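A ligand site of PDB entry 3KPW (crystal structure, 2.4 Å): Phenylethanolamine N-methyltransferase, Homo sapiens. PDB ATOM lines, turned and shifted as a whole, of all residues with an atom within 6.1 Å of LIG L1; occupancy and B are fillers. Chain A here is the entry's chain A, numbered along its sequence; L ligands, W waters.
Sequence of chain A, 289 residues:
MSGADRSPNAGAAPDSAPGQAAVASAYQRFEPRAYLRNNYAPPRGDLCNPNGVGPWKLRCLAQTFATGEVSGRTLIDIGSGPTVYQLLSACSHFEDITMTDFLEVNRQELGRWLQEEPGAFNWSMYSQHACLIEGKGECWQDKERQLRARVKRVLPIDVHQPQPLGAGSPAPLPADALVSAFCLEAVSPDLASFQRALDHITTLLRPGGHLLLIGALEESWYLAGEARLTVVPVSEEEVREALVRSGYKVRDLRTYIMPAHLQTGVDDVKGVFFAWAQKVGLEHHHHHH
S1 of LIG L1 lies close to O of Phe 182 (3.6 Å). CE2 of Tyr 27 touches C8 of LIG L1, 3.6 Å away. Gly 81 touches LIG L1 (CA to O4, 3.1 Å). Thr 83 touches LIG L1. Gln 86 touches LIG L1 (NE2 to N1, 3.6 Å). Phe 102 touches LIG L1. Leu 103 touches LIG L1. Ile 157 touches LIG L1 (O to C13, 3.8 Å). Val 187 touches LIG L1. Tyr 222 touches LIG L1 (OH to C5, 3.9998 Å). Hydrophobic or aromatic side chains within 4 Å of LIG L1: Tyr 27, Tyr 35, Tyr 40, Tyr 85, Phe 102, Leu 103, Val 159, His 160, Ala 181, Phe 182 and Val 187. Within 4 Å of LIG L1: Tyr 27, Tyr 35, Tyr 40, Gly 79, Ser 80, Gly 81, Thr 83, Tyr 85, Gln 86, Asp 101, Phe 102, Leu 103, Asn 106, Ile 157, Asp 158, Val 159, His 160, Ala 181, Phe 182, Cys 183, Val 187 and Tyr 222. The nearest printed residue that does not touch LIG L1 is Phe 30 (4.2 Å).
The side-chain carboxylate of Asp 101 lies close to the side-chain amide oxygen of Asn 106 (3.1 Å). OH of Tyr 40 is in hydrogen-bond range of NZ of Lys 57, 3.1 Å away. O of Ser 80 lies within hydrogen-bond range of NE2 of Gln 86, at 3.4 Å. O of Asp 101 sits at hydrogen-bond distance from N of Ile 157, at 3.3 Å. The side-chain hydroxyl (OH) of Tyr 27 sits at hydrogen-bond distance from the backbone carbonyl oxygen (O) of Ala 186 (2.6 Å). N of Leu 103 sits at hydrogen-bond distance from OD2 of Asp 101, 3.1 Å away. The side-chain hydroxyl of Tyr 85 is in hydrogen-bond range of the side-chain amino group of Lys 57, 3.2 Å away. NE2 of His 160 lies close to O of Val 187 (3.1 Å).
Water W2 lies within hydrogen-bond range of NE2 of His 160 (3.0 Å) and N4 of LIG L1 (3.5 Å).
OD1 of Asn 106 sits at hydrogen-bond distance from O4 of LIG L1 (3.0 Å). An oxygen (O2) of LIG L1 lies within hydrogen-bond range of the side-chain hydroxyl of Tyr 35 (2.6 Å). The side-chain hydroxyl (OH) of Tyr 85 lies within hydrogen-bond range of an oxygen (O1) of LIG L1 (2.7 Å). The side-chain carboxylate (OD1) of Asp 101 lies within hydrogen-bond range of an oxygen (O4) of LIG L1, at 2.8 Å. O of Ser 80 lies within hydrogen-bond range of N1 of LIG L1 (3.1 Å). A nitrogen (N6) of LIG L1 lies within hydrogen-bond range of the side-chain sulfur (SG) of Cys 183, at 3.5 Å. N4 of LIG L1 is in hydrogen-bond range of OD1 of Asp 158 (3.1 Å). The backbone NH (N) of Val 159 sits at hydrogen-bond distance from a nitrogen (N5) of LIG L1. N4 of LIG L1 lies close to NE2 of His 160 (3.4 Å). A nitrogen (N1) of LIG L1 lies within hydrogen-bond range of the backbone carbonyl oxygen of Ala 181. N1 of LIG L1 sits at hydrogen-bond distance from O of Gly 79 (2.8 Å). O2 of LIG L1 sits at hydrogen-bond distance from OH of Tyr 40, 2.7 Å away.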
ATOM      1  N   ALA A  24       5.144 -34.916 -30.231  1.00  0.00           N
ATOM      2  CA  ALA A  24       5.955 -35.748 -29.362  1.00  0.00           C
ATOM      3  C   ALA A  24       7.191 -36.276 -30.081  1.00  0.00           C
ATOM      4  O   ALA A  24       8.292 -35.720 -29.969  1.00  0.00           O
ATOM      5  CB  ALA A  24       5.122 -36.909 -28.795  1.00  0.00           C
ATOM      6  N   TYR A  27       8.429 -33.916 -32.873  1.00  0.00           N
ATOM      7  CA  TYR A  27       9.378 -32.871 -32.535  1.00  0.00           C
ATOM      8  C   TYR A  27      10.805 -33.348 -32.645  1.00  0.00           C
ATOM      9  O   TYR A  27      11.733 -32.581 -32.392  1.00  0.00           O
ATOM     10  CB  TYR A  27       9.090 -32.280 -31.147  1.00  0.00           C
ATOM     11  CG  TYR A  27       8.083 -31.152 -31.238  1.00  0.00           C
ATOM     12  CD1 TYR A  27       6.744 -31.358 -30.978  1.00  0.00           C
ATOM     13  CD2 TYR A  27       8.493 -29.889 -31.651  1.00  0.00           C
ATOM     14  CE1 TYR A  27       5.834 -30.329 -31.072  1.00  0.00           C
ATOM     15  CE2 TYR A  27       7.592 -28.849 -31.764  1.00  0.00           C
ATOM     16  CZ  TYR A  27       6.268 -29.067 -31.480  1.00  0.00           C
ATOM     17  OH  TYR A  27       5.377 -28.038 -31.606  1.00  0.00           O
ATOM     18  N   PHE A  30      12.249 -31.845 -35.728  1.00  0.00           N
ATOM     19  CA  PHE A  30      12.191 -30.384 -35.699  1.00  0.00           C
ATOM     20  C   PHE A  30      13.561 -29.735 -35.983  1.00  0.00           C
ATOM     21  O   PHE A  30      14.486 -29.885 -35.189  1.00  0.00           O
ATOM     22  CB  PHE A  30      11.651 -29.951 -34.334  1.00  0.00           C
ATOM     23  CG  PHE A  30      11.535 -28.465 -34.135  1.00  0.00           C
ATOM     24  CD1 PHE A  30      10.292 -27.845 -34.095  1.00  0.00           C
ATOM     25  CD2 PHE A  30      12.671 -27.689 -33.936  1.00  0.00           C
ATOM     26  CE1 PHE A  30      10.184 -26.481 -33.876  1.00  0.00           C
ATOM     27  CE2 PHE A  30      12.563 -26.325 -33.717  1.00  0.00           C
ATOM     28  CZ  PHE A  30      11.325 -25.725 -33.686  1.00  0.00           C
ATOM     29  N   TYR A  35      12.939 -23.579 -38.723  1.00  0.00           N
ATOM     30  CA  TYR A  35      11.882 -22.880 -38.006  1.00  0.00           C
ATOM     31  C   TYR A  35      12.144 -21.371 -38.002  1.00  0.00           C
ATOM     32  O   TYR A  35      11.262 -20.588 -38.345  1.00  0.00           O
ATOM     33  CB  TYR A  35      11.715 -23.423 -36.588  1.00  0.00           C
ATOM     34  CG  TYR A  35      10.728 -22.632 -35.735  1.00  0.00           C
ATOM     35  CD1 TYR A  35       9.351 -22.860 -35.806  1.00  0.00           C
ATOM     36  CD2 TYR A  35      11.181 -21.663 -34.841  1.00  0.00           C
ATOM     37  CE1 TYR A  35       8.441 -22.141 -35.014  1.00  0.00           C
ATOM     38  CE2 TYR A  35      10.278 -20.932 -34.038  1.00  0.00           C
ATOM     39  CZ  TYR A  35       8.927 -21.175 -34.137  1.00  0.00           C
ATOM     40  OH  TYR A  35       8.077 -20.465 -33.334  1.00  0.00           O
ATOM     41  N   ASN A  39       9.846 -18.355 -39.896  1.00  0.00           N
ATOM     42  CA  ASN A  39       9.069 -17.451 -39.047  1.00  0.00           C
ATOM     43  C   ASN A  39       9.731 -16.136 -38.671  1.00  0.00           C
ATOM     44  O   ASN A  39       9.062 -15.209 -38.181  1.00  0.00           O
ATOM     45  CB  ASN A  39       8.595 -18.164 -37.784  1.00  0.00           C
ATOM     46  CG  ASN A  39       7.701 -19.360 -38.097  1.00  0.00           C
ATOM     47  OD1 ASN A  39       6.535 -19.205 -38.416  1.00  0.00           O
ATOM     48  ND2 ASN A  39       8.265 -20.539 -38.033  1.00  0.00           N
ATOM     49  N   TYR A  40      11.039 -16.047 -38.900  1.00  0.00           N
ATOM     50  CA  TYR A  40      11.812 -14.952 -38.358  1.00  0.00           C
ATOM     51  C   TYR A  40      12.761 -14.396 -39.394  1.00  0.00           C
ATOM     52  O   TYR A  40      13.620 -13.610 -39.073  1.00  0.00           O
ATOM     53  CB  TYR A  40      12.515 -15.391 -37.076  1.00  0.00           C
ATOM     54  CG  TYR A  40      11.507 -15.668 -35.992  1.00  0.00           C
ATOM     55  CD1 TYR A  40      11.129 -16.973 -35.673  1.00  0.00           C
ATOM     56  CD2 TYR A  40      10.858 -14.620 -35.340  1.00  0.00           C
ATOM     57  CE1 TYR A  40      10.165 -17.217 -34.692  1.00  0.00           C
ATOM     58  CE2 TYR A  40       9.906 -14.852 -34.408  1.00  0.00           C
ATOM     59  CZ  TYR A  40       9.558 -16.146 -34.074  1.00  0.00           C
ATOM     60  OH  TYR A  40       8.603 -16.323 -33.099  1.00  0.00           O
ATOM     61  N   LYS A  57       3.953  -8.187 -32.236  1.00  0.00           N
ATOM     62  CA  LYS A  57       4.383  -8.924 -31.059  1.00  0.00           C
ATOM     63  C   LYS A  57       5.285  -8.076 -30.153  1.00  0.00           C
ATOM     64  O   LYS A  57       5.031  -7.971 -28.949  1.00  0.00           O
ATOM     65  CB  LYS A  57       5.078 -10.207 -31.460  1.00  0.00           C
ATOM     66  CG  LYS A  57       4.135 -11.202 -32.125  1.00  0.00           C
ATOM     67  CD  LYS A  57       4.741 -12.599 -32.179  1.00  0.00           C
ATOM     68  CE  LYS A  57       5.996 -12.652 -33.057  1.00  0.00           C
ATOM     69  NZ  LYS A  57       6.515 -14.028 -33.204  1.00  0.00           N
ATOM     70  N   ASP A  77      10.986 -18.306 -19.218  1.00  0.00           N
ATOM     71  CA  ASP A  77      10.441 -18.365 -20.568  1.00  0.00           C
ATOM     72  C   ASP A  77      10.201 -19.827 -20.915  1.00  0.00           C
ATOM     73  O   ASP A  77      11.154 -20.620 -20.917  1.00  0.00           O
ATOM     74  CB  ASP A  77      11.400 -17.711 -21.590  1.00  0.00           C
ATOM     75  CG  ASP A  77      10.839 -17.696 -23.004  1.00  0.00           C
ATOM     76  OD1 ASP A  77       9.637 -17.417 -23.178  1.00  0.00           O
ATOM     77  OD2 ASP A  77      11.599 -17.961 -23.968  1.00  0.00           O
ATOM     78  N   ILE A  78       8.934 -20.159 -21.181  1.00  0.00           N
ATOM     79  CA  ILE A  78       8.478 -21.538 -21.403  1.00  0.00           C
ATOM     80  C   ILE A  78       8.447 -21.858 -22.877  1.00  0.00           C
ATOM     81  O   ILE A  78       7.726 -21.204 -23.635  1.00  0.00           O
ATOM     82  CB  ILE A  78       7.010 -21.709 -20.933  1.00  0.00           C
ATOM     83  CG1 ILE A  78       6.793 -21.121 -19.529  1.00  0.00           C
ATOM     84  CG2 ILE A  78       6.588 -23.180 -21.043  1.00  0.00           C
ATOM     85  CD1 ILE A  78       7.554 -21.803 -18.440  1.00  0.00           C
ATOM     86  N   GLY A  79       9.182 -22.884 -23.285  1.00  0.00           N
ATOM     87  CA  GLY A  79       9.182 -23.281 -24.679  1.00  0.00           C
ATOM     88  C   GLY A  79       9.843 -22.240 -25.570  1.00  0.00           C
ATOM     89  O   GLY A  79       9.303 -21.843 -26.612  1.00  0.00           O
ATOM     90  N   SER A  80      11.029 -21.805 -25.163  1.00  0.00           N
ATOM     91  CA  SER A  80      11.750 -20.732 -25.826  1.00  0.00           C
ATOM     92  C   SER A  80      12.006 -21.030 -27.284  1.00  0.00           C
ATOM     93  O   SER A  80      12.103 -20.102 -28.105  1.00  0.00           O
ATOM     94  CB  SER A  80      13.096 -20.531 -25.136  1.00  0.00           C
ATOM     95  OG  SER A  80      12.904 -20.236 -23.780  1.00  0.00           O
ATOM     96  N   GLY A  81      12.129 -22.314 -27.595  1.00  0.00           N
ATOM     97  CA  GLY A  81      12.677 -22.722 -28.880  1.00  0.00           C
ATOM     98  C   GLY A  81      14.062 -22.110 -29.103  1.00  0.00           C
ATOM     99  O   GLY A  81      14.856 -21.967 -28.175  1.00  0.00           O
ATOM    100  N   PRO A  82      14.355 -21.719 -30.341  1.00  0.00           N
ATOM    101  CA  PRO A  82      15.634 -21.090 -30.669  1.00  0.00           C
ATOM    102  C   PRO A  82      15.473 -19.570 -30.795  1.00  0.00           C
ATOM    103  O   PRO A  82      16.162 -18.964 -31.604  1.00  0.00           O
ATOM    104  CB  PRO A  82      15.939 -21.666 -32.056  1.00  0.00           C
ATOM    105  CG  PRO A  82      14.551 -22.071 -32.629  1.00  0.00           C
ATOM    106  CD  PRO A  82      13.524 -21.890 -31.545  1.00  0.00           C
ATOM    107  N   THR A  83      14.546 -18.979 -30.044  1.00  0.00           N
ATOM    108  CA  THR A  83      14.276 -17.552 -30.243  1.00  0.00           C
ATOM    109  C   THR A  83      14.451 -16.744 -28.945  1.00  0.00           C
ATOM    110  O   THR A  83      14.188 -17.254 -27.845  1.00  0.00           O
ATOM    111  CB  THR A  83      12.899 -17.302 -30.938  1.00  0.00           C
ATOM    112  OG1 THR A  83      11.804 -17.442 -30.004  1.00  0.00           O
ATOM    113  CG2 THR A  83      12.690 -18.261 -32.128  1.00  0.00           C
ATOM    114  N   TYR A  85      13.629 -13.057 -29.012  1.00  0.00           N
ATOM    115  CA  TYR A  85      12.926 -11.781 -29.187  1.00  0.00           C
ATOM    116  C   TYR A  85      11.921 -11.550 -28.098  1.00  0.00           C
ATOM    117  O   TYR A  85      11.593 -10.399 -27.793  1.00  0.00           O
ATOM    118  CB  TYR A  85      12.164 -11.745 -30.520  1.00  0.00           C
ATOM    119  CG  TYR A  85      10.969 -12.676 -30.533  1.00  0.00           C
ATOM    120  CD1 TYR A  85       9.706 -12.217 -30.220  1.00  0.00           C
ATOM    121  CD2 TYR A  85      11.120 -14.035 -30.832  1.00  0.00           C
ATOM    122  CE1 TYR A  85       8.613 -13.047 -30.222  1.00  0.00           C
ATOM    123  CE2 TYR A  85      10.022 -14.887 -30.835  1.00  0.00           C
ATOM    124  CZ  TYR A  85       8.786 -14.383 -30.523  1.00  0.00           C
ATOM    125  OH  TYR A  85       7.693 -15.209 -30.511  1.00  0.00           O
ATOM    126  N   GLN A  86      11.403 -12.644 -27.547  1.00  0.00           N
ATOM    127  CA  GLN A  86      10.280 -12.571 -26.622  1.00  0.00           C
ATOM    128  C   GLN A  86      10.723 -12.104 -25.250  1.00  0.00           C
ATOM    129  O   GLN A  86       9.894 -11.937 -24.368  1.00  0.00           O
ATOM    130  CB  GLN A  86       9.521 -13.905 -26.537  1.00  0.00           C
ATOM    131  CG  GLN A  86      10.266 -15.112 -25.927  1.00  0.00           C
ATOM    132  CD  GLN A  86      11.078 -15.910 -26.938  1.00  0.00           C
ATOM    133  OE1 GLN A  86      11.467 -15.406 -28.004  1.00  0.00           O
ATOM    134  NE2 GLN A  86      11.374 -17.153 -26.597  1.00  0.00           N
ATOM    135  N   ASP A 101      13.520 -25.221 -23.111  1.00  0.00           N
ATOM    136  CA  ASP A 101      12.856 -25.895 -24.212  1.00  0.00           C
ATOM    137  C   ASP A 101      12.962 -27.390 -24.044  1.00  0.00           C
ATOM    138  O   ASP A 101      13.824 -27.886 -23.325  1.00  0.00           O
ATOM    139  CB  ASP A 101      13.421 -25.508 -25.566  1.00  0.00           C
ATOM    140  CG  ASP A 101      12.453 -25.797 -26.684  1.00  0.00           C
ATOM    141  OD1 ASP A 101      11.365 -25.174 -26.706  1.00  0.00           O
ATOM    142  OD2 ASP A 101      12.796 -26.639 -27.544  1.00  0.00           O
ATOM    143  N   PHE A 102      12.072 -28.084 -24.745  1.00  0.00           N
ATOM    144  CA  PHE A 102      12.026 -29.537 -24.729  1.00  0.00           C
ATOM    145  C   PHE A 102      13.185 -30.147 -25.534  1.00  0.00           C
ATOM    146  O   PHE A 102      13.676 -31.222 -25.212  1.00  0.00           O
ATOM    147  CB  PHE A 102      10.660 -29.970 -25.273  1.00  0.00           C
ATOM    148  CG  PHE A 102      10.450 -31.453 -25.320  1.00  0.00           C
ATOM    149  CD1 PHE A 102      10.196 -32.173 -24.166  1.00  0.00           C
ATOM    150  CD2 PHE A 102      10.466 -32.128 -26.529  1.00  0.00           C
ATOM    151  CE1 PHE A 102       9.987 -33.546 -24.216  1.00  0.00           C
ATOM    152  CE2 PHE A 102      10.267 -33.499 -26.588  1.00  0.00           C
ATOM    153  CZ  PHE A 102      10.013 -34.205 -25.431  1.00  0.00           C
ATOM    154  N   LEU A 103      13.639 -29.438 -26.572  1.00  0.00           N
ATOM    155  CA  LEU A 103      14.663 -29.984 -27.472  1.00  0.00           C
ATOM    156  C   LEU A 103      16.100 -29.544 -27.160  1.00  0.00           C
ATOM    157  O   LEU A 103      16.382 -28.360 -26.957  1.00  0.00           O
ATOM    158  CB  LEU A 103      14.345 -29.657 -28.931  1.00  0.00           C
ATOM    159  CG  LEU A 103      13.134 -30.349 -29.541  1.00  0.00           C
ATOM    160  CD1 LEU A 103      12.878 -29.903 -30.975  1.00  0.00           C
ATOM    161  CD2 LEU A 103      13.306 -31.870 -29.467  1.00  0.00           C
ATOM    162  N   ASN A 106      17.391 -27.056 -29.847  1.00  0.00           N
ATOM    163  CA  ASN A 106      16.975 -25.687 -29.575  1.00  0.00           C
ATOM    164  C   ASN A 106      17.787 -25.055 -28.469  1.00  0.00           C
ATOM    165  O   ASN A 106      18.152 -23.894 -28.557  1.00  0.00           O
ATOM    166  CB  ASN A 106      15.499 -25.602 -29.232  1.00  0.00           C
ATOM    167  CG  ASN A 106      14.636 -25.458 -30.446  1.00  0.00           C
ATOM    168  OD1 ASN A 106      13.424 -25.671 -30.390  1.00  0.00           O
ATOM    169  ND2 ASN A 106      15.258 -25.111 -31.571  1.00  0.00           N
ATOM    170  N   ILE A 157      12.613 -28.810 -20.423  1.00  0.00           N
ATOM    171  CA  ILE A 157      11.304 -28.690 -19.827  1.00  0.00           C
ATOM    172  C   ILE A 157      10.317 -29.493 -20.656  1.00  0.00           C
ATOM    173  O   ILE A 157      10.506 -29.638 -21.878  1.00  0.00           O
ATOM    174  CB  ILE A 157      10.851 -27.221 -19.788  1.00  0.00           C
ATOM    175  CG1 ILE A 157       9.481 -27.084 -19.116  1.00  0.00           C
ATOM    176  CG2 ILE A 157      10.840 -26.616 -21.207  1.00  0.00           C
ATOM    177  CD1 ILE A 157       9.134 -25.668 -18.732  1.00  0.00           C
ATOM    178  N   ASP A 158       9.294 -30.025 -19.990  1.00  0.00           N
ATOM    179  CA  ASP A 158       8.158 -30.683 -20.647  1.00  0.00           C
ATOM    180  C   ASP A 158       6.874 -30.239 -19.971  1.00  0.00           C
ATOM    181  O   ASP A 158       6.653 -30.531 -18.778  1.00  0.00           O
ATOM    182  CB  ASP A 158       8.268 -32.209 -20.558  1.00  0.00           C
ATOM    183  CG  ASP A 158       7.083 -32.915 -21.196  1.00  0.00           C
ATOM    184  OD1 ASP A 158       6.050 -32.260 -21.440  1.00  0.00           O
ATOM    185  OD2 ASP A 158       7.190 -34.127 -21.475  1.00  0.00           O
ATOM    186  N   VAL A 159       6.020 -29.556 -20.710  1.00  0.00           N
ATOM    187  CA  VAL A 159       4.817 -28.977 -20.135  1.00  0.00           C
ATOM    188  C   VAL A 159       3.748 -30.033 -19.864  1.00  0.00           C
ATOM    189  O   VAL A 159       2.807 -29.779 -19.108  1.00  0.00           O
ATOM    190  CB  VAL A 159       4.218 -27.895 -21.034  1.00  0.00           C
ATOM    191  CG1 VAL A 159       5.170 -26.710 -21.124  1.00  0.00           C
ATOM    192  CG2 VAL A 159       3.892 -28.471 -22.400  1.00  0.00           C
ATOM    193  N   HIS A 160       3.889 -31.201 -20.472  1.00  0.00           N
ATOM    194  CA  HIS A 160       3.008 -32.310 -20.153  1.00  0.00           C
ATOM    195  C   HIS A 160       3.243 -32.833 -18.730  1.00  0.00           C
ATOM    196  O   HIS A 160       2.319 -33.387 -18.120  1.00  0.00           O
ATOM    197  CB  HIS A 160       3.170 -33.429 -21.170  1.00  0.00           C
ATOM    198  CG  HIS A 160       2.980 -32.966 -22.579  1.00  0.00           C
ATOM    199  ND1 HIS A 160       1.981 -32.092 -22.944  1.00  0.00           N
ATOM    200  CD2 HIS A 160       3.669 -33.245 -23.702  1.00  0.00           C
ATOM    201  CE1 HIS A 160       2.059 -31.857 -24.239  1.00  0.00           C
ATOM    202  NE2 HIS A 160       3.067 -32.553 -24.729  1.00  0.00           N
ATOM    203  N   SER A 180       5.538 -17.056 -22.475  1.00  0.00           N
ATOM    204  CA  SER A 180       5.555 -18.218 -23.353  1.00  0.00           C
ATOM    205  C   SER A 180       4.949 -17.915 -24.701  1.00  0.00           C
ATOM    206  O   SER A 180       3.789 -17.476 -24.808  1.00  0.00           O
ATOM    207  CB  SER A 180       4.835 -19.406 -22.730  1.00  0.00           C
ATOM    208  OG  SER A 180       4.988 -20.530 -23.574  1.00  0.00           O
ATOM    209  N   ALA A 181       5.722 -18.168 -25.744  1.00  0.00           N
ATOM    210  CA  ALA A 181       5.289 -17.826 -27.091  1.00  0.00           C
ATOM    211  C   ALA A 181       5.207 -19.043 -27.987  1.00  0.00           C
ATOM    212  O   ALA A 181       6.218 -19.741 -28.203  1.00  0.00           O
ATOM    213  CB  ALA A 181       6.219 -16.755 -27.701  1.00  0.00           C
ATOM    214  N   PHE A 182       4.012 -19.300 -28.498  1.00  0.00           N
ATOM    215  CA  PHE A 182       3.834 -20.338 -29.512  1.00  0.00           C
ATOM    216  C   PHE A 182       4.190 -21.762 -29.020  1.00  0.00           C
ATOM    217  O   PHE A 182       4.547 -22.640 -29.818  1.00  0.00           O
ATOM    218  CB  PHE A 182       4.638 -19.980 -30.763  1.00  0.00           C
ATOM    219  CG  PHE A 182       4.236 -18.676 -31.393  1.00  0.00           C
ATOM    220  CD1 PHE A 182       5.061 -17.567 -31.298  1.00  0.00           C
ATOM    221  CD2 PHE A 182       3.025 -18.555 -32.052  1.00  0.00           C
ATOM    222  CE1 PHE A 182       4.679 -16.346 -31.883  1.00  0.00           C
ATOM    223  CE2 PHE A 182       2.644 -17.363 -32.644  1.00  0.00           C
ATOM    224  CZ  PHE A 182       3.474 -16.259 -32.555  1.00  0.00           C
ATOM    225  N   CYS A 183       4.073 -21.992 -27.715  1.00  0.00           N
ATOM    226  CA  CYS A 183       4.360 -23.319 -27.178  1.00  0.00           C
ATOM    227  C   CYS A 183       3.125 -24.198 -27.017  1.00  0.00           C
ATOM    228  O   CYS A 183       2.935 -25.165 -27.754  1.00  0.00           O
ATOM    229  CB  CYS A 183       5.082 -23.217 -25.844  1.00  0.00           C
ATOM    230  SG  CYS A 183       5.756 -24.792 -25.280  1.00  0.00           S
ATOM    231  N   ALA A 186       1.006 -25.574 -29.723  1.00  0.00           N
ATOM    232  CA  ALA A 186       1.908 -26.280 -30.629  1.00  0.00           C
ATOM    233  C   ALA A 186       2.351 -27.641 -30.120  1.00  0.00           C
ATOM    234  O   ALA A 186       2.913 -28.424 -30.879  1.00  0.00           O
ATOM    235  CB  ALA A 186       3.148 -25.409 -30.907  1.00  0.00           C
ATOM    236  N   VAL A 187       2.147 -27.921 -28.828  1.00  0.00           N
ATOM    237  CA  VAL A 187       2.566 -29.204 -28.251  1.00  0.00           C
ATOM    238  C   VAL A 187       1.382 -30.019 -27.721  1.00  0.00           C
ATOM    239  O   VAL A 187       1.567 -31.000 -26.995  1.00  0.00           O
ATOM    240  CB  VAL A 187       3.609 -29.020 -27.116  1.00  0.00           C
ATOM    241  CG1 VAL A 187       4.775 -28.189 -27.597  1.00  0.00           C
ATOM    242  CG2 VAL A 187       2.973 -28.370 -25.902  1.00  0.00           C
ATOM    243  N   TYR A 222       2.158 -26.745 -38.637  1.00  0.00           N
ATOM    244  CA  TYR A 222       3.206 -25.881 -39.167  1.00  0.00           C
ATOM    245  C   TYR A 222       4.413 -26.778 -39.418  1.00  0.00           C
ATOM    246  O   TYR A 222       4.472 -27.901 -38.925  1.00  0.00           O
ATOM    247  CB  TYR A 222       3.530 -24.733 -38.209  1.00  0.00           C
ATOM    248  CG  TYR A 222       4.285 -25.132 -36.967  1.00  0.00           C
ATOM    249  CD1 TYR A 222       5.637 -24.817 -36.838  1.00  0.00           C
ATOM    250  CD2 TYR A 222       3.663 -25.845 -35.925  1.00  0.00           C
ATOM    251  CE1 TYR A 222       6.355 -25.183 -35.705  1.00  0.00           C
ATOM    252  CE2 TYR A 222       4.384 -26.216 -34.769  1.00  0.00           C
ATOM    253  CZ  TYR A 222       5.729 -25.876 -34.684  1.00  0.00           C
ATOM    254  OH  TYR A 222       6.497 -26.179 -33.598  1.00  0.00           O
HETATM  255  N1  LIG L   1       9.107 -19.524 -28.145  1.00  0.00           N
HETATM  256  C1  LIG L   1       9.339 -19.813 -29.551  1.00  0.00           C
HETATM  257  C2  LIG L   1       8.344 -20.915 -29.956  1.00  0.00           C
HETATM  258  C3  LIG L   1       9.115 -22.136 -30.428  1.00  0.00           C
HETATM  259  S1  LIG L   1       7.856 -23.190 -31.228  1.00  0.00           S
HETATM  260  C4  LIG L   1       8.923 -18.585 -30.379  1.00  0.00           C
HETATM  261  O1  LIG L   1       8.112 -17.841 -29.924  1.00  0.00           O
HETATM  262  O2  LIG L   1       9.027 -18.658 -31.755  1.00  0.00           O
HETATM  263  C5  LIG L   1       7.189 -24.426 -30.070  1.00  0.00           C
HETATM  264  C6  LIG L   1       8.261 -24.952 -29.097  1.00  0.00           C
HETATM  265  O3  LIG L   1       7.689 -25.926 -28.176  1.00  0.00           O
HETATM  266  C7  LIG L   1       9.430 -25.658 -29.809  1.00  0.00           C
HETATM  267  O4  LIG L   1      10.633 -25.024 -29.441  1.00  0.00           O
HETATM  268  C8  LIG L   1       9.390 -27.053 -29.217  1.00  0.00           C
HETATM  269  O5  LIG L   1      10.595 -27.757 -29.213  1.00  0.00           O
HETATM  270  C9  LIG L   1       8.803 -26.817 -27.825  1.00  0.00           C
HETATM  271  N2  LIG L   1       8.277 -28.065 -27.301  1.00  0.00           N
HETATM  272  C10 LIG L   1       7.965 -29.292 -28.081  1.00  0.00           C
HETATM  273  N3  LIG L   1       7.411 -30.274 -27.151  1.00  0.00           N
HETATM  274  C11 LIG L   1       7.361 -29.668 -25.814  1.00  0.00           C
HETATM  275  C12 LIG L   1       6.886 -30.212 -24.497  1.00  0.00           C
HETATM  276  N4  LIG L   1       6.331 -31.564 -24.414  1.00  0.00           N
HETATM  277  N5  LIG L   1       6.959 -29.369 -23.318  1.00  0.00           N
HETATM  278  C13 LIG L   1       7.510 -27.969 -23.415  1.00  0.00           C
HETATM  279  N6  LIG L   1       7.999 -27.442 -24.721  1.00  0.00           N
HETATM  280  C14 LIG L   1       7.896 -28.296 -25.916  1.00  0.00           C
HETATM  281  N1  LG2 L   2       2.024 -19.183 -36.878  1.00  0.00           N
HETATM  282  C1  LG2 L   2       3.259 -19.169 -36.113  1.00  0.00           C
HETATM  283  N2  LG2 L   2       3.711 -20.347 -35.460  1.00  0.00           N
HETATM  284  C2  LG2 L   2       4.928 -20.320 -34.689  1.00  0.00           C
HETATM  285  C3  LG2 L   2       5.683 -19.107 -34.604  1.00  0.00           C
HETATM  286  C4  LG2 L   2       5.206 -17.919 -35.273  1.00  0.00           C
HETATM  287  C5  LG2 L   2       5.944 -16.693 -35.181  1.00  0.00           C
HETATM  288  C6  LG2 L   2       5.461 -15.476 -35.881  1.00  0.00           C
HETATM  289  C7  LG2 L   2       4.252 -15.500 -36.630  1.00  0.00           C
HETATM  290  C8  LG2 L   2       3.521 -16.714 -36.711  1.00  0.00           C
HETATM  291  C9  LG2 L   2       4.015 -17.939 -36.011  1.00  0.00           C
HETATM  292  O   HOH W   1       6.135 -32.880 -27.375  1.00  0.00           O
HETATM  293  O   HOH W   2       5.147 -34.591 -25.596  1.00  0.00           O
